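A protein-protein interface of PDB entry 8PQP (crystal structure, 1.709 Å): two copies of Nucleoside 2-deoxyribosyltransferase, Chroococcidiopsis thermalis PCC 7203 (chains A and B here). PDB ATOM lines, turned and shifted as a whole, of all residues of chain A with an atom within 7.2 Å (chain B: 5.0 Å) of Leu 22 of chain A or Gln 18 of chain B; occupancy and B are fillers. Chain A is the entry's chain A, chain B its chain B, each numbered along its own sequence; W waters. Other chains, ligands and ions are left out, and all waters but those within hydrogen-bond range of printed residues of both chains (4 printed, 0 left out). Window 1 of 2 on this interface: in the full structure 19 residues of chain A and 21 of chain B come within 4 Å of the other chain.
The side-chain hydroxyl (OG) of Ser 15 of chain B lies within hydrogen-bond range of the backbone NH (N) of Gln 18 of chain B (3.2 Å). O of Gln 18 of chain A is in hydrogen-bond range of N of Leu 23 of chain A (3.4 Å). The side-chain hydroxyl of Tyr 12 of chain A is in hydrogen-bond range of the side-chain amide nitrogen of Asn 77 of chain A, at 2.8 Å. The backbone carbonyl oxygen (O) of Tyr 12 of chain B sits at hydrogen-bond distance from the backbone NH (N) of Lys 19 of chain B. The backbone carbonyl oxygen (O) of Gln 17 of chain B lies within hydrogen-bond range of the side-chain hydroxyl (OG1) of Thr 20 of chain B, 3.1 Å away. The side-chain hydroxyl (OG) of Ser 15 of chain B sits close to the backbone NH (N) of Gln 17 of chain B (3.4 Å).
Water W4 lies within hydrogen-bond range of the side-chain amide oxygen of Gln 17 of chain B (2.4 Å), the side-chain hydroxyl of Tyr 12 of chain A (2.9 Å) and the side-chain carboxylate of Asp 104 of chain A (3.2 Å). Water W3 lies within hydrogen-bond range of OE1 of Gln 17 of chain A (2.5 Å) and OH of Tyr 12 of chain B (2.7 Å). Water W2 lies within hydrogen-bond range of OD2 of Asp 104 of chain A (2.9 Å), NE2 of Gln 16 of chain B (3.0 Å) and N of Val 138 of chain A (3.1 Å). Water W1 lies within hydrogen-bond range of NE2 of Gln 16 of chain B and N of Val 138 of chain A.
Among the printed residues, merely in contact across the chains: Leu 21 of chain A with Leu 21 of chain B (3.5 Å), Leu 22 of chain A with Gln 18 of chain B (3.7 Å), Gln 18 of chain A with Leu 22 of chain B (3.7 Å), Val 138 of chain A with Gln 17 of chain B (3.7 Å), Ile 26 of chain A with Gln 17 of chain B (3.8 Å), Pro 25 of chain A with Gln 17 of chain B (3.8 Å) and Leu 22 of chain A with Leu 21 of chain B (3.99 Å).
Printed residues of chain B within 4 Å of Leu 22 of chain A: Gln 17 (2.9 Å), Gln 18 (3.7 Å) and Leu 21 (3.99 Å). Of the printed residues of chain B, Asp 104 of chain A touches Ser 15, Gln 16 and Gln 17. Of the printed residues of chain A, Tyr 12 of chain B touches Gln 18. Of the printed residues of chain A, Gln 16 of chain B touches Asp 104. Of the printed residues of chain A, Leu 21 of chain B touches Leu 21 (3.5 Å) and Leu 22 (3.99 Å). The nearest printed residue of chain B that does not touch Val 138 of chain A is Gln 16 of chain B (4.8 Å).
Hydrophobic or aromatic side chains of chain B within 4 Å of the printed part of chain A: Tyr 12, Leu 21 and Leu 22. Along chain B the printed residues that touch a printed residue of chain A span positions 12 to 22. Of the 21 printed residues of chain A, 9 touch a printed residue of chain B. Hydrophobic or aromatic side chains of chain A that line the printed part of chain B: Tyr 12, Leu 21, Leu 22, Pro 25, Ile 26 and Val 138.
Tyr 12 of chain A touches Gln 18 of chain B, and with the chains exchanged Gln 18 of chain A touches Tyr 12 of chain B. Gln 17 of chain A touches Leu 22 of chain B, and with the chains exchanged Leu 22 of chain A touches Gln 17 of chain B. Gln 18 of chain A touches Leu 22 of chain B, and with the chains exchanged Leu 22 of chain A touches Gln 18 of chain B. Leu 22 of chain A touches Leu 21 of chain B, but with the chains exchanged Leu 21 of chain A does not touch Leu 22 of chain B (4.03 Å). Positions printed for both chains: 11, 12, 16, 17, 18, 19, 20, 21, 22 and 23.
The side-chain amide nitrogen (NE2) of Gln 18 of chain A sits at hydrogen-bond distance from the side-chain hydroxyl (OH) of Tyr 12 of chain B (3.2 Å). N of Gln 17 of chain B sits at hydrogen-bond distance from OD2 of Asp 104 of chain A (3.0 Å). The backbone carbonyl oxygen (O) of Leu 22 of chain B lies within hydrogen-bond range of the side-chain amide nitrogen (NE2) of Gln 17 of chain A, at 3.0 Å. OH of Tyr 12 of chain A is in hydrogen-bond range of NE2 of Gln 18 of chain B. O of Asp 104 of chain A lies within hydrogen-bond range of N of Gln 16 of chain B. OD1 of Asp 104 of chain A lies within hydrogen-bond range of OG of Ser 15 of chain B, 2.8 Å away. The backbone carbonyl oxygen (O) of Leu 22 of chain A is in hydrogen-bond range of the side-chain amide nitrogen (NE2) of Gln 17 of chain B, 2.9 Å away.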
ATOM      1  N   PRO A  11     -27.015   6.410  18.655  1.00  0.00           N
ATOM      2  CA  PRO A  11     -28.086   5.986  17.735  1.00  0.00           C
ATOM      3  C   PRO A  11     -27.583   5.279  16.485  1.00  0.00           C
ATOM      4  O   PRO A  11     -28.373   5.052  15.560  1.00  0.00           O
ATOM      5  CB  PRO A  11     -28.730   7.324  17.354  1.00  0.00           C
ATOM      6  CG  PRO A  11     -27.530   8.265  17.289  1.00  0.00           C
ATOM      7  CD  PRO A  11     -26.592   7.802  18.400  1.00  0.00           C
ATOM      8  N   TYR A  12     -26.289   4.949  16.442  1.00  0.00           N
ATOM      9  CA  TYR A  12     -25.674   4.466  15.216  1.00  0.00           C
ATOM     10  C   TYR A  12     -26.114   3.056  14.874  1.00  0.00           C
ATOM     11  O   TYR A  12     -26.020   2.649  13.708  1.00  0.00           O
ATOM     12  CB  TYR A  12     -24.155   4.564  15.341  1.00  0.00           C
ATOM     13  CG  TYR A  12     -23.670   5.992  15.228  1.00  0.00           C
ATOM     14  CD1 TYR A  12     -24.532   7.007  14.810  1.00  0.00           C
ATOM     15  CD2 TYR A  12     -22.363   6.336  15.540  1.00  0.00           C
ATOM     16  CE1 TYR A  12     -24.097   8.322  14.684  1.00  0.00           C
ATOM     17  CE2 TYR A  12     -21.922   7.647  15.413  1.00  0.00           C
ATOM     18  CZ  TYR A  12     -22.786   8.633  14.989  1.00  0.00           C
ATOM     19  OH  TYR A  12     -22.343   9.933  14.861  1.00  0.00           O
ATOM     20  N   GLN A  16     -27.881   0.870   8.995  1.00  0.00           N
ATOM     21  CA  GLN A  16     -26.935  -0.178   8.614  1.00  0.00           C
ATOM     22  C   GLN A  16     -25.539   0.393   8.386  1.00  0.00           C
ATOM     23  O   GLN A  16     -24.549  -0.130   8.914  1.00  0.00           O
ATOM     24  CB  GLN A  16     -27.418  -0.915   7.366  1.00  0.00           C
ATOM     25  CG  GLN A  16     -26.676  -2.223   7.142  1.00  0.00           C
ATOM     26  CD  GLN A  16     -25.893  -2.249   5.837  1.00  0.00           C
ATOM     27  OE1 GLN A  16     -26.383  -1.809   4.794  1.00  0.00           O
ATOM     28  NE2 GLN A  16     -24.665  -2.765   5.893  1.00  0.00           N
ATOM     29  N   GLN A  17     -25.447   1.485   7.618  1.00  0.00           N
ATOM     30  CA  GLN A  17     -24.146   2.066   7.291  1.00  0.00           C
ATOM     31  C   GLN A  17     -23.445   2.617   8.530  1.00  0.00           C
ATOM     32  O   GLN A  17     -22.247   2.388   8.725  1.00  0.00           O
ATOM     33  CB  GLN A  17     -24.308   3.165   6.242  1.00  0.00           C
ATOM     34  CG  GLN A  17     -23.217   3.173   5.179  1.00  0.00           C
ATOM     35  CD  GLN A  17     -23.142   4.499   4.438  1.00  0.00           C
ATOM     36  OE1 GLN A  17     -23.939   5.406   4.695  1.00  0.00           O
ATOM     37  NE2 GLN A  17     -22.187   4.621   3.521  1.00  0.00           N
ATOM     38  N   GLN A  18     -24.163   3.373   9.363  1.00  0.00           N
ATOM     39  CA  GLN A  18     -23.519   3.999  10.515  1.00  0.00           C
ATOM     40  C   GLN A  18     -23.047   2.953  11.517  1.00  0.00           C
ATOM     41  O   GLN A  18     -21.978   3.103  12.122  1.00  0.00           O
ATOM     42  CB  GLN A  18     -24.467   4.984  11.198  1.00  0.00           C
ATOM     43  CG  GLN A  18     -24.966   6.122  10.292  1.00  0.00           C
ATOM     44  CD  GLN A  18     -26.130   6.905  10.902  1.00  0.00           C
ATOM     45  OE1 GLN A  18     -26.442   6.768  12.090  1.00  0.00           O
ATOM     46  NE2 GLN A  18     -26.769   7.740  10.082  1.00  0.00           N
ATOM     47  N   LYS A  19     -23.836   1.895  11.705  1.00  0.00           N
ATOM     48  CA  LYS A  19     -23.435   0.812  12.597  1.00  0.00           C
ATOM     49  C   LYS A  19     -22.167   0.139  12.093  1.00  0.00           C
ATOM     50  O   LYS A  19     -21.287  -0.227  12.881  1.00  0.00           O
ATOM     51  CB  LYS A  19     -24.576  -0.201  12.706  1.00  0.00           C
ATOM     52  CG  LYS A  19     -24.246  -1.442  13.510  1.00  0.00           C
ATOM     53  CD  LYS A  19     -25.398  -2.428  13.455  1.00  0.00           C
ATOM     54  CE  LYS A  19     -25.013  -3.726  14.150  1.00  0.00           C
ATOM     55  NZ  LYS A  19     -26.181  -4.392  14.776  1.00  0.00           N
ATOM     56  N   THR A  20     -22.051  -0.012  10.773  1.00  0.00           N
ATOM     57  CA  THR A  20     -20.926  -0.694  10.150  1.00  0.00           C
ATOM     58  C   THR A  20     -19.676   0.182  10.120  1.00  0.00           C
ATOM     59  O   THR A  20     -18.563  -0.313  10.326  1.00  0.00           O
ATOM     60  CB  THR A  20     -21.321  -1.117   8.727  1.00  0.00           C
ATOM     61  OG1 THR A  20     -22.313  -2.149   8.795  1.00  0.00           O
ATOM     62  CG2 THR A  20     -20.120  -1.617   7.939  1.00  0.00           C
ATOM     63  N   LEU A  21     -19.833   1.483   9.875  1.00  0.00           N
ATOM     64  CA  LEU A  21     -18.703   2.362   9.594  1.00  0.00           C
ATOM     65  C   LEU A  21     -18.345   3.296  10.735  1.00  0.00           C
ATOM     66  O   LEU A  21     -17.160   3.535  10.980  1.00  0.00           O
ATOM     67  CB  LEU A  21     -18.983   3.205   8.350  1.00  0.00           C
ATOM     68  CG  LEU A  21     -19.158   2.441   7.043  1.00  0.00           C
ATOM     69  CD1 LEU A  21     -19.247   3.417   5.873  1.00  0.00           C
ATOM     70  CD2 LEU A  21     -18.009   1.474   6.831  1.00  0.00           C
ATOM     71  N   LEU A  22     -19.331   3.847  11.440  1.00  0.00           N
ATOM     72  CA  LEU A  22     -19.019   4.838  12.459  1.00  0.00           C
ATOM     73  C   LEU A  22     -18.653   4.201  13.796  1.00  0.00           C
ATOM     74  O   LEU A  22     -17.760   4.701  14.487  1.00  0.00           O
ATOM     75  CB  LEU A  22     -20.192   5.797  12.655  1.00  0.00           C
ATOM     76  CG  LEU A  22     -20.651   6.538  11.395  1.00  0.00           C
ATOM     77  CD1 LEU A  22     -21.731   7.539  11.781  1.00  0.00           C
ATOM     78  CD2 LEU A  22     -19.482   7.235  10.728  1.00  0.00           C
ATOM     79  N   LEU A  23     -19.329   3.113  14.186  1.00  0.00           N
ATOM     80  CA  LEU A  23     -19.127   2.583  15.538  1.00  0.00           C
ATOM     81  C   LEU A  23     -17.752   1.944  15.728  1.00  0.00           C
ATOM     82  O   LEU A  23     -17.098   2.255  16.736  1.00  0.00           O
ATOM     83  CB  LEU A  23     -20.257   1.616  15.906  1.00  0.00           C
ATOM     84  CG  LEU A  23     -21.485   2.287  16.531  1.00  0.00           C
ATOM     85  CD1 LEU A  23     -22.642   1.301  16.781  1.00  0.00           C
ATOM     86  CD2 LEU A  23     -21.101   3.015  17.807  1.00  0.00           C
ATOM     87  N   PRO A  24     -17.255   1.073  14.843  1.00  0.00           N
ATOM     88  CA  PRO A  24     -15.974   0.383  15.112  1.00  0.00           C
ATOM     89  C   PRO A  24     -14.831   1.342  15.414  1.00  0.00           C
ATOM     90  O   PRO A  24     -14.066   1.093  16.361  1.00  0.00           O
ATOM     91  CB  PRO A  24     -15.727  -0.413  13.821  1.00  0.00           C
ATOM     92  CG  PRO A  24     -17.090  -0.727  13.365  1.00  0.00           C
ATOM     93  CD  PRO A  24     -17.886   0.520  13.630  1.00  0.00           C
ATOM     94  N   PRO A  25     -14.667   2.451  14.680  1.00  0.00           N
ATOM     95  CA  PRO A  25     -13.565   3.363  15.044  1.00  0.00           C
ATOM     96  C   PRO A  25     -13.692   3.960  16.439  1.00  0.00           C
ATOM     97  O   PRO A  25     -12.666   4.225  17.076  1.00  0.00           O
ATOM     98  CB  PRO A  25     -13.625   4.445  13.958  1.00  0.00           C
ATOM     99  CG  PRO A  25     -14.273   3.778  12.806  1.00  0.00           C
ATOM    100  CD  PRO A  25     -15.285   2.858  13.399  1.00  0.00           C
ATOM    101  N   ILE A  26     -14.914   4.191  16.933  1.00  0.00           N
ATOM    102  CA  ILE A  26     -15.085   4.725  18.282  1.00  0.00           C
ATOM    103  C   ILE A  26     -14.819   3.645  19.320  1.00  0.00           C
ATOM    104  O   ILE A  26     -14.167   3.893  20.340  1.00  0.00           O
ATOM    105  CB  ILE A  26     -16.498   5.321  18.450  1.00  0.00           C
ATOM    106  CG1 ILE A  26     -16.679   6.519  17.520  1.00  0.00           C
ATOM    107  CG2 ILE A  26     -16.764   5.677  19.950  1.00  0.00           C
ATOM    108  CD1 ILE A  26     -18.130   6.878  17.281  1.00  0.00           C
ATOM    109  N   VAL A  27     -15.315   2.429  19.077  1.00  0.00           N
ATOM    110  CA  VAL A  27     -15.017   1.305  19.963  1.00  0.00           C
ATOM    111  C   VAL A  27     -13.511   1.097  20.070  1.00  0.00           C
ATOM    112  O   VAL A  27     -12.959   0.899  21.158  1.00  0.00           O
ATOM    113  CB  VAL A  27     -15.721   0.034  19.455  1.00  0.00           C
ATOM    114  CG1 VAL A  27     -15.219  -1.189  20.215  1.00  0.00           C
ATOM    115  CG2 VAL A  27     -17.248   0.189  19.553  1.00  0.00           C
ATOM    116  N   VAL A  75     -22.856   9.426  22.428  1.00  0.00           N
ATOM    117  CA  VAL A  75     -22.821  10.106  21.139  1.00  0.00           C
ATOM    118  C   VAL A  75     -24.060  10.994  21.068  1.00  0.00           C
ATOM    119  O   VAL A  75     -25.187  10.500  20.983  1.00  0.00           O
ATOM    120  CB  VAL A  75     -22.776   9.104  19.987  1.00  0.00           C
ATOM    121  CG1 VAL A  75     -22.894   9.818  18.618  1.00  0.00           C
ATOM    122  CG2 VAL A  75     -21.480   8.282  20.080  1.00  0.00           C
ATOM    123  N   ASN A  77     -24.619  13.472  18.777  1.00  0.00           N
ATOM    124  CA  ASN A  77     -24.810  14.066  17.466  1.00  0.00           C
ATOM    125  C   ASN A  77     -26.302  14.194  17.148  1.00  0.00           C
ATOM    126  O   ASN A  77     -27.147  13.545  17.762  1.00  0.00           O
ATOM    127  CB  ASN A  77     -24.131  13.218  16.387  1.00  0.00           C
ATOM    128  CG  ASN A  77     -22.648  13.484  16.300  1.00  0.00           C
ATOM    129  OD1 ASN A  77     -22.195  14.559  16.660  1.00  0.00           O
ATOM    130  ND2 ASN A  77     -21.888  12.506  15.834  1.00  0.00           N
ATOM    131  N   GLY A  78     -26.617  15.037  16.172  1.00  0.00           N
ATOM    132  CA  GLY A  78     -27.989  15.184  15.733  1.00  0.00           C
ATOM    133  C   GLY A  78     -28.660  16.424  16.308  1.00  0.00           C
ATOM    134  O   GLY A  78     -28.190  17.049  17.260  1.00  0.00           O
ATOM    135  N   ASP A 104     -19.395  15.442  17.034  1.00  0.00           N
ATOM    136  CA  ASP A 104     -18.608  16.008  15.941  1.00  0.00           C
ATOM    137  C   ASP A 104     -19.496  16.685  14.896  1.00  0.00           C
ATOM    138  O   ASP A 104     -19.052  16.956  13.773  1.00  0.00           O
ATOM    139  CB  ASP A 104     -17.709  14.940  15.315  1.00  0.00           C
ATOM    140  CG  ASP A 104     -18.484  13.827  14.629  1.00  0.00           C
ATOM    141  OD1 ASP A 104     -19.736  13.827  14.667  1.00  0.00           O
ATOM    142  OD2 ASP A 104     -17.818  12.957  14.020  1.00  0.00           O
ATOM    143  N   ASP A 105     -20.739  16.960  15.269  1.00  0.00           N
ATOM    144  CA  ASP A 105     -21.720  17.701  14.481  1.00  0.00           C
ATOM    145  C   ASP A 105     -21.455  19.190  14.677  1.00  0.00           C
ATOM    146  O   ASP A 105     -21.429  19.663  15.816  1.00  0.00           O
ATOM    147  CB  ASP A 105     -23.110  17.288  14.988  1.00  0.00           C
ATOM    148  CG  ASP A 105     -24.278  17.880  14.196  1.00  0.00           C
ATOM    149  OD1 ASP A 105     -24.102  18.829  13.403  1.00  0.00           O
ATOM    150  OD2 ASP A 105     -25.410  17.382  14.416  1.00  0.00           O
ATOM    151  N   ARG A 107     -23.303  21.732  13.855  1.00  0.00           N
ATOM    152  CA  ARG A 107     -24.466  22.594  14.006  1.00  0.00           C
ATOM    153  C   ARG A 107     -24.619  23.009  15.464  1.00  0.00           C
ATOM    154  O   ARG A 107     -24.318  22.239  16.381  1.00  0.00           O
ATOM    155  CB  ARG A 107     -25.730  21.895  13.513  1.00  0.00           C
ATOM    156  CG  ARG A 107     -25.823  21.828  12.011  1.00  0.00           C
ATOM    157  CD  ARG A 107     -26.914  20.897  11.581  1.00  0.00           C
ATOM    158  NE  ARG A 107     -26.712  19.577  12.153  1.00  0.00           N
ATOM    159  CZ  ARG A 107     -27.550  18.564  11.984  1.00  0.00           C
ATOM    160  NH1 ARG A 107     -28.658  18.726  11.259  1.00  0.00           N
ATOM    161  NH2 ARG A 107     -27.283  17.392  12.539  1.00  0.00           N
ATOM    162  N   VAL A 138     -13.265  11.918  16.663  1.00  0.00           N
ATOM    163  CA  VAL A 138     -12.845  10.574  17.053  1.00  0.00           C
ATOM    164  C   VAL A 138     -11.365  10.563  17.419  1.00  0.00           C
ATOM    165  O   VAL A 138     -10.947   9.876  18.364  1.00  0.00           O
ATOM    166  CB  VAL A 138     -13.161   9.565  15.930  1.00  0.00           C
ATOM    167  CG1 VAL A 138     -12.755   8.156  16.351  1.00  0.00           C
ATOM    168  CG2 VAL A 138     -14.645   9.600  15.591  1.00  0.00           C
ATOM    169  N   PRO B  11     -27.781  14.974   5.361  1.00  0.00           N
ATOM    170  CA  PRO B  11     -27.219  15.700   6.506  1.00  0.00           C
ATOM    171  C   PRO B  11     -25.807  15.259   6.878  1.00  0.00           C
ATOM    172  O   PRO B  11     -25.317  15.672   7.935  1.00  0.00           O
ATOM    173  CB  PRO B  11     -28.196  15.324   7.624  1.00  0.00           C
ATOM    174  CG  PRO B  11     -28.473  13.871   7.344  1.00  0.00           C
ATOM    175  CD  PRO B  11     -28.545  13.787   5.800  1.00  0.00           C
ATOM    176  N   TYR B  12     -25.172  14.428   6.049  1.00  0.00           N
ATOM    177  CA  TYR B  12     -23.937  13.764   6.449  1.00  0.00           C
ATOM    178  C   TYR B  12     -22.746  14.711   6.481  1.00  0.00           C
ATOM    179  O   TYR B  12     -21.748  14.405   7.143  1.00  0.00           O
ATOM    180  CB  TYR B  12     -23.680  12.573   5.522  1.00  0.00           C
ATOM    181  CG  TYR B  12     -24.544  11.370   5.861  1.00  0.00           C
ATOM    182  CD1 TYR B  12     -25.284  11.337   7.046  1.00  0.00           C
ATOM    183  CD2 TYR B  12     -24.609  10.267   5.018  1.00  0.00           C
ATOM    184  CE1 TYR B  12     -26.067  10.245   7.377  1.00  0.00           C
ATOM    185  CE2 TYR B  12     -25.396   9.160   5.346  1.00  0.00           C
ATOM    186  CZ  TYR B  12     -26.125   9.161   6.526  1.00  0.00           C
ATOM    187  OH  TYR B  12     -26.903   8.078   6.865  1.00  0.00           O
ATOM    188  N   SER B  15     -21.514  16.218  10.255  1.00  0.00           N
ATOM    189  CA  SER B  15     -20.654  15.488  11.178  1.00  0.00           C
ATOM    190  C   SER B  15     -19.358  15.098  10.479  1.00  0.00           C
ATOM    191  O   SER B  15     -19.376  14.621   9.339  1.00  0.00           O
ATOM    192  CB  SER B  15     -21.370  14.244  11.709  1.00  0.00           C
ATOM    193  OG  SER B  15     -20.457  13.228  12.077  1.00  0.00           O
ATOM    194  N   GLN B  16     -18.236  15.314  11.170  1.00  0.00           N
ATOM    195  CA  GLN B  16     -16.919  15.016  10.606  1.00  0.00           C
ATOM    196  C   GLN B  16     -16.795  13.549  10.215  1.00  0.00           C
ATOM    197  O   GLN B  16     -16.331  13.226   9.116  1.00  0.00           O
ATOM    198  CB  GLN B  16     -15.825  15.390  11.610  1.00  0.00           C
ATOM    199  CG  GLN B  16     -14.415  15.473  11.009  1.00  0.00           C
ATOM    200  CD  GLN B  16     -13.310  15.465  12.060  1.00  0.00           C
ATOM    201  OE1 GLN B  16     -12.767  16.511  12.421  1.00  0.00           O
ATOM    202  NE2 GLN B  16     -12.961  14.276  12.543  1.00  0.00           N
ATOM    203  N   GLN B  17     -17.203  12.640  11.105  1.00  0.00           N
ATOM    204  CA  GLN B  17     -17.091  11.219  10.791  1.00  0.00           C
ATOM    205  C   GLN B  17     -18.083  10.813   9.709  1.00  0.00           C
ATOM    206  O   GLN B  17     -17.747  10.023   8.816  1.00  0.00           O
ATOM    207  CB  GLN B  17     -17.301  10.383  12.055  1.00  0.00           C
ATOM    208  CG  GLN B  17     -16.557   9.059  12.072  1.00  0.00           C
ATOM    209  CD  GLN B  17     -17.061   8.128  13.171  1.00  0.00           C
ATOM    210  OE1 GLN B  17     -18.059   8.424  13.838  1.00  0.00           O
ATOM    211  NE2 GLN B  17     -16.390   6.987  13.346  1.00  0.00           N
ATOM    212  N   GLN B  18     -19.313  11.332   9.771  1.00  0.00           N
ATOM    213  CA  GLN B  18     -20.289  11.018   8.726  1.00  0.00           C
ATOM    214  C   GLN B  18     -19.838  11.559   7.374  1.00  0.00           C
ATOM    215  O   GLN B  18     -19.934  10.863   6.356  1.00  0.00           O
ATOM    216  CB  GLN B  18     -21.666  11.571   9.104  1.00  0.00           C
ATOM    217  CG  GLN B  18     -22.265  10.841  10.314  1.00  0.00           C
ATOM    218  CD  GLN B  18     -23.473  11.547  10.889  1.00  0.00           C
ATOM    219  OE1 GLN B  18     -24.197  12.238  10.173  1.00  0.00           O
ATOM    220  NE2 GLN B  18     -23.693  11.384  12.190  1.00  0.00           N
ATOM    221  N   LYS B  19     -19.325  12.790   7.349  1.00  0.00           N
ATOM    222  CA  LYS B  19     -18.845  13.378   6.095  1.00  0.00           C
ATOM    223  C   LYS B  19     -17.743  12.534   5.463  1.00  0.00           C
ATOM    224  O   LYS B  19     -17.744  12.295   4.248  1.00  0.00           O
ATOM    225  CB  LYS B  19     -18.343  14.799   6.349  1.00  0.00           C
ATOM    226  CG  LYS B  19     -17.735  15.479   5.133  1.00  0.00           C
ATOM    227  CD  LYS B  19     -17.354  16.914   5.455  1.00  0.00           C
ATOM    228  CE  LYS B  19     -16.629  17.563   4.283  1.00  0.00           C
ATOM    229  NZ  LYS B  19     -17.436  18.654   3.673  1.00  0.00           N
ATOM    230  N   THR B  20     -16.788  12.075   6.277  1.00  0.00           N
ATOM    231  CA  THR B  20     -15.626  11.370   5.748  1.00  0.00           C
ATOM    232  C   THR B  20     -15.920   9.910   5.427  1.00  0.00           C
ATOM    233  O   THR B  20     -15.313   9.357   4.504  1.00  0.00           O
ATOM    234  CB  THR B  20     -14.459  11.428   6.748  1.00  0.00           C
ATOM    235  OG1 THR B  20     -14.825  10.725   7.934  1.00  0.00           O
ATOM    236  CG2 THR B  20     -14.110  12.860   7.119  1.00  0.00           C
ATOM    237  N   LEU B  21     -16.817   9.261   6.176  1.00  0.00           N
ATOM    238  CA  LEU B  21     -17.004   7.814   6.081  1.00  0.00           C
ATOM    239  C   LEU B  21     -18.267   7.400   5.334  1.00  0.00           C
ATOM    240  O   LEU B  21     -18.225   6.444   4.561  1.00  0.00           O
ATOM    241  CB  LEU B  21     -17.029   7.189   7.482  1.00  0.00           C
ATOM    242  CG  LEU B  21     -15.715   7.234   8.265  1.00  0.00           C
ATOM    243  CD1 LEU B  21     -15.793   6.341   9.490  1.00  0.00           C
ATOM    244  CD2 LEU B  21     -14.568   6.817   7.365  1.00  0.00           C
ATOM    245  N   LEU B  22     -19.396   8.072   5.549  1.00  0.00           N
ATOM    246  CA  LEU B  22     -20.652   7.625   4.951  1.00  0.00           C
ATOM    247  C   LEU B  22     -20.866   8.145   3.532  1.00  0.00           C
ATOM    248  O   LEU B  22     -21.431   7.437   2.696  1.00  0.00           O
ATOM    249  CB  LEU B  22     -21.837   8.063   5.807  1.00  0.00           C
ATOM    250  CG  LEU B  22     -21.785   7.713   7.297  1.00  0.00           C
ATOM    251  CD1 LEU B  22     -23.059   8.218   7.946  1.00  0.00           C
ATOM    252  CD2 LEU B  22     -21.654   6.223   7.471  1.00  0.00           C
ATOM    253  N   LEU B  23     -20.460   9.389   3.258  1.00  0.00           N
ATOM    254  CA  LEU B  23     -20.784   9.998   1.966  1.00  0.00           C
ATOM    255  C   LEU B  23     -20.016   9.384   0.804  1.00  0.00           C
ATOM    256  O   LEU B  23     -20.634   9.140  -0.249  1.00  0.00           O
ATOM    257  CB  LEU B  23     -20.557  11.510   2.036  1.00  0.00           C
ATOM    258  CG  LEU B  23     -21.784  12.368   2.287  1.00  0.00           C
ATOM    259  CD1 LEU B  23     -21.359  13.779   2.650  1.00  0.00           C
ATOM    260  CD2 LEU B  23     -22.657  12.352   1.043  1.00  0.00           C
HETATM  261  O   HOH W   1     -11.290  12.219  13.928  1.00  0.00           O
HETATM  262  O   HOH W   2     -14.972  12.859  14.192  1.00  0.00           O
HETATM  263  O   HOH W   3     -26.177   5.750   5.669  1.00  0.00           O
HETATM  264  O   HOH W   4     -19.516  10.254  14.401  1.00  0.00           O
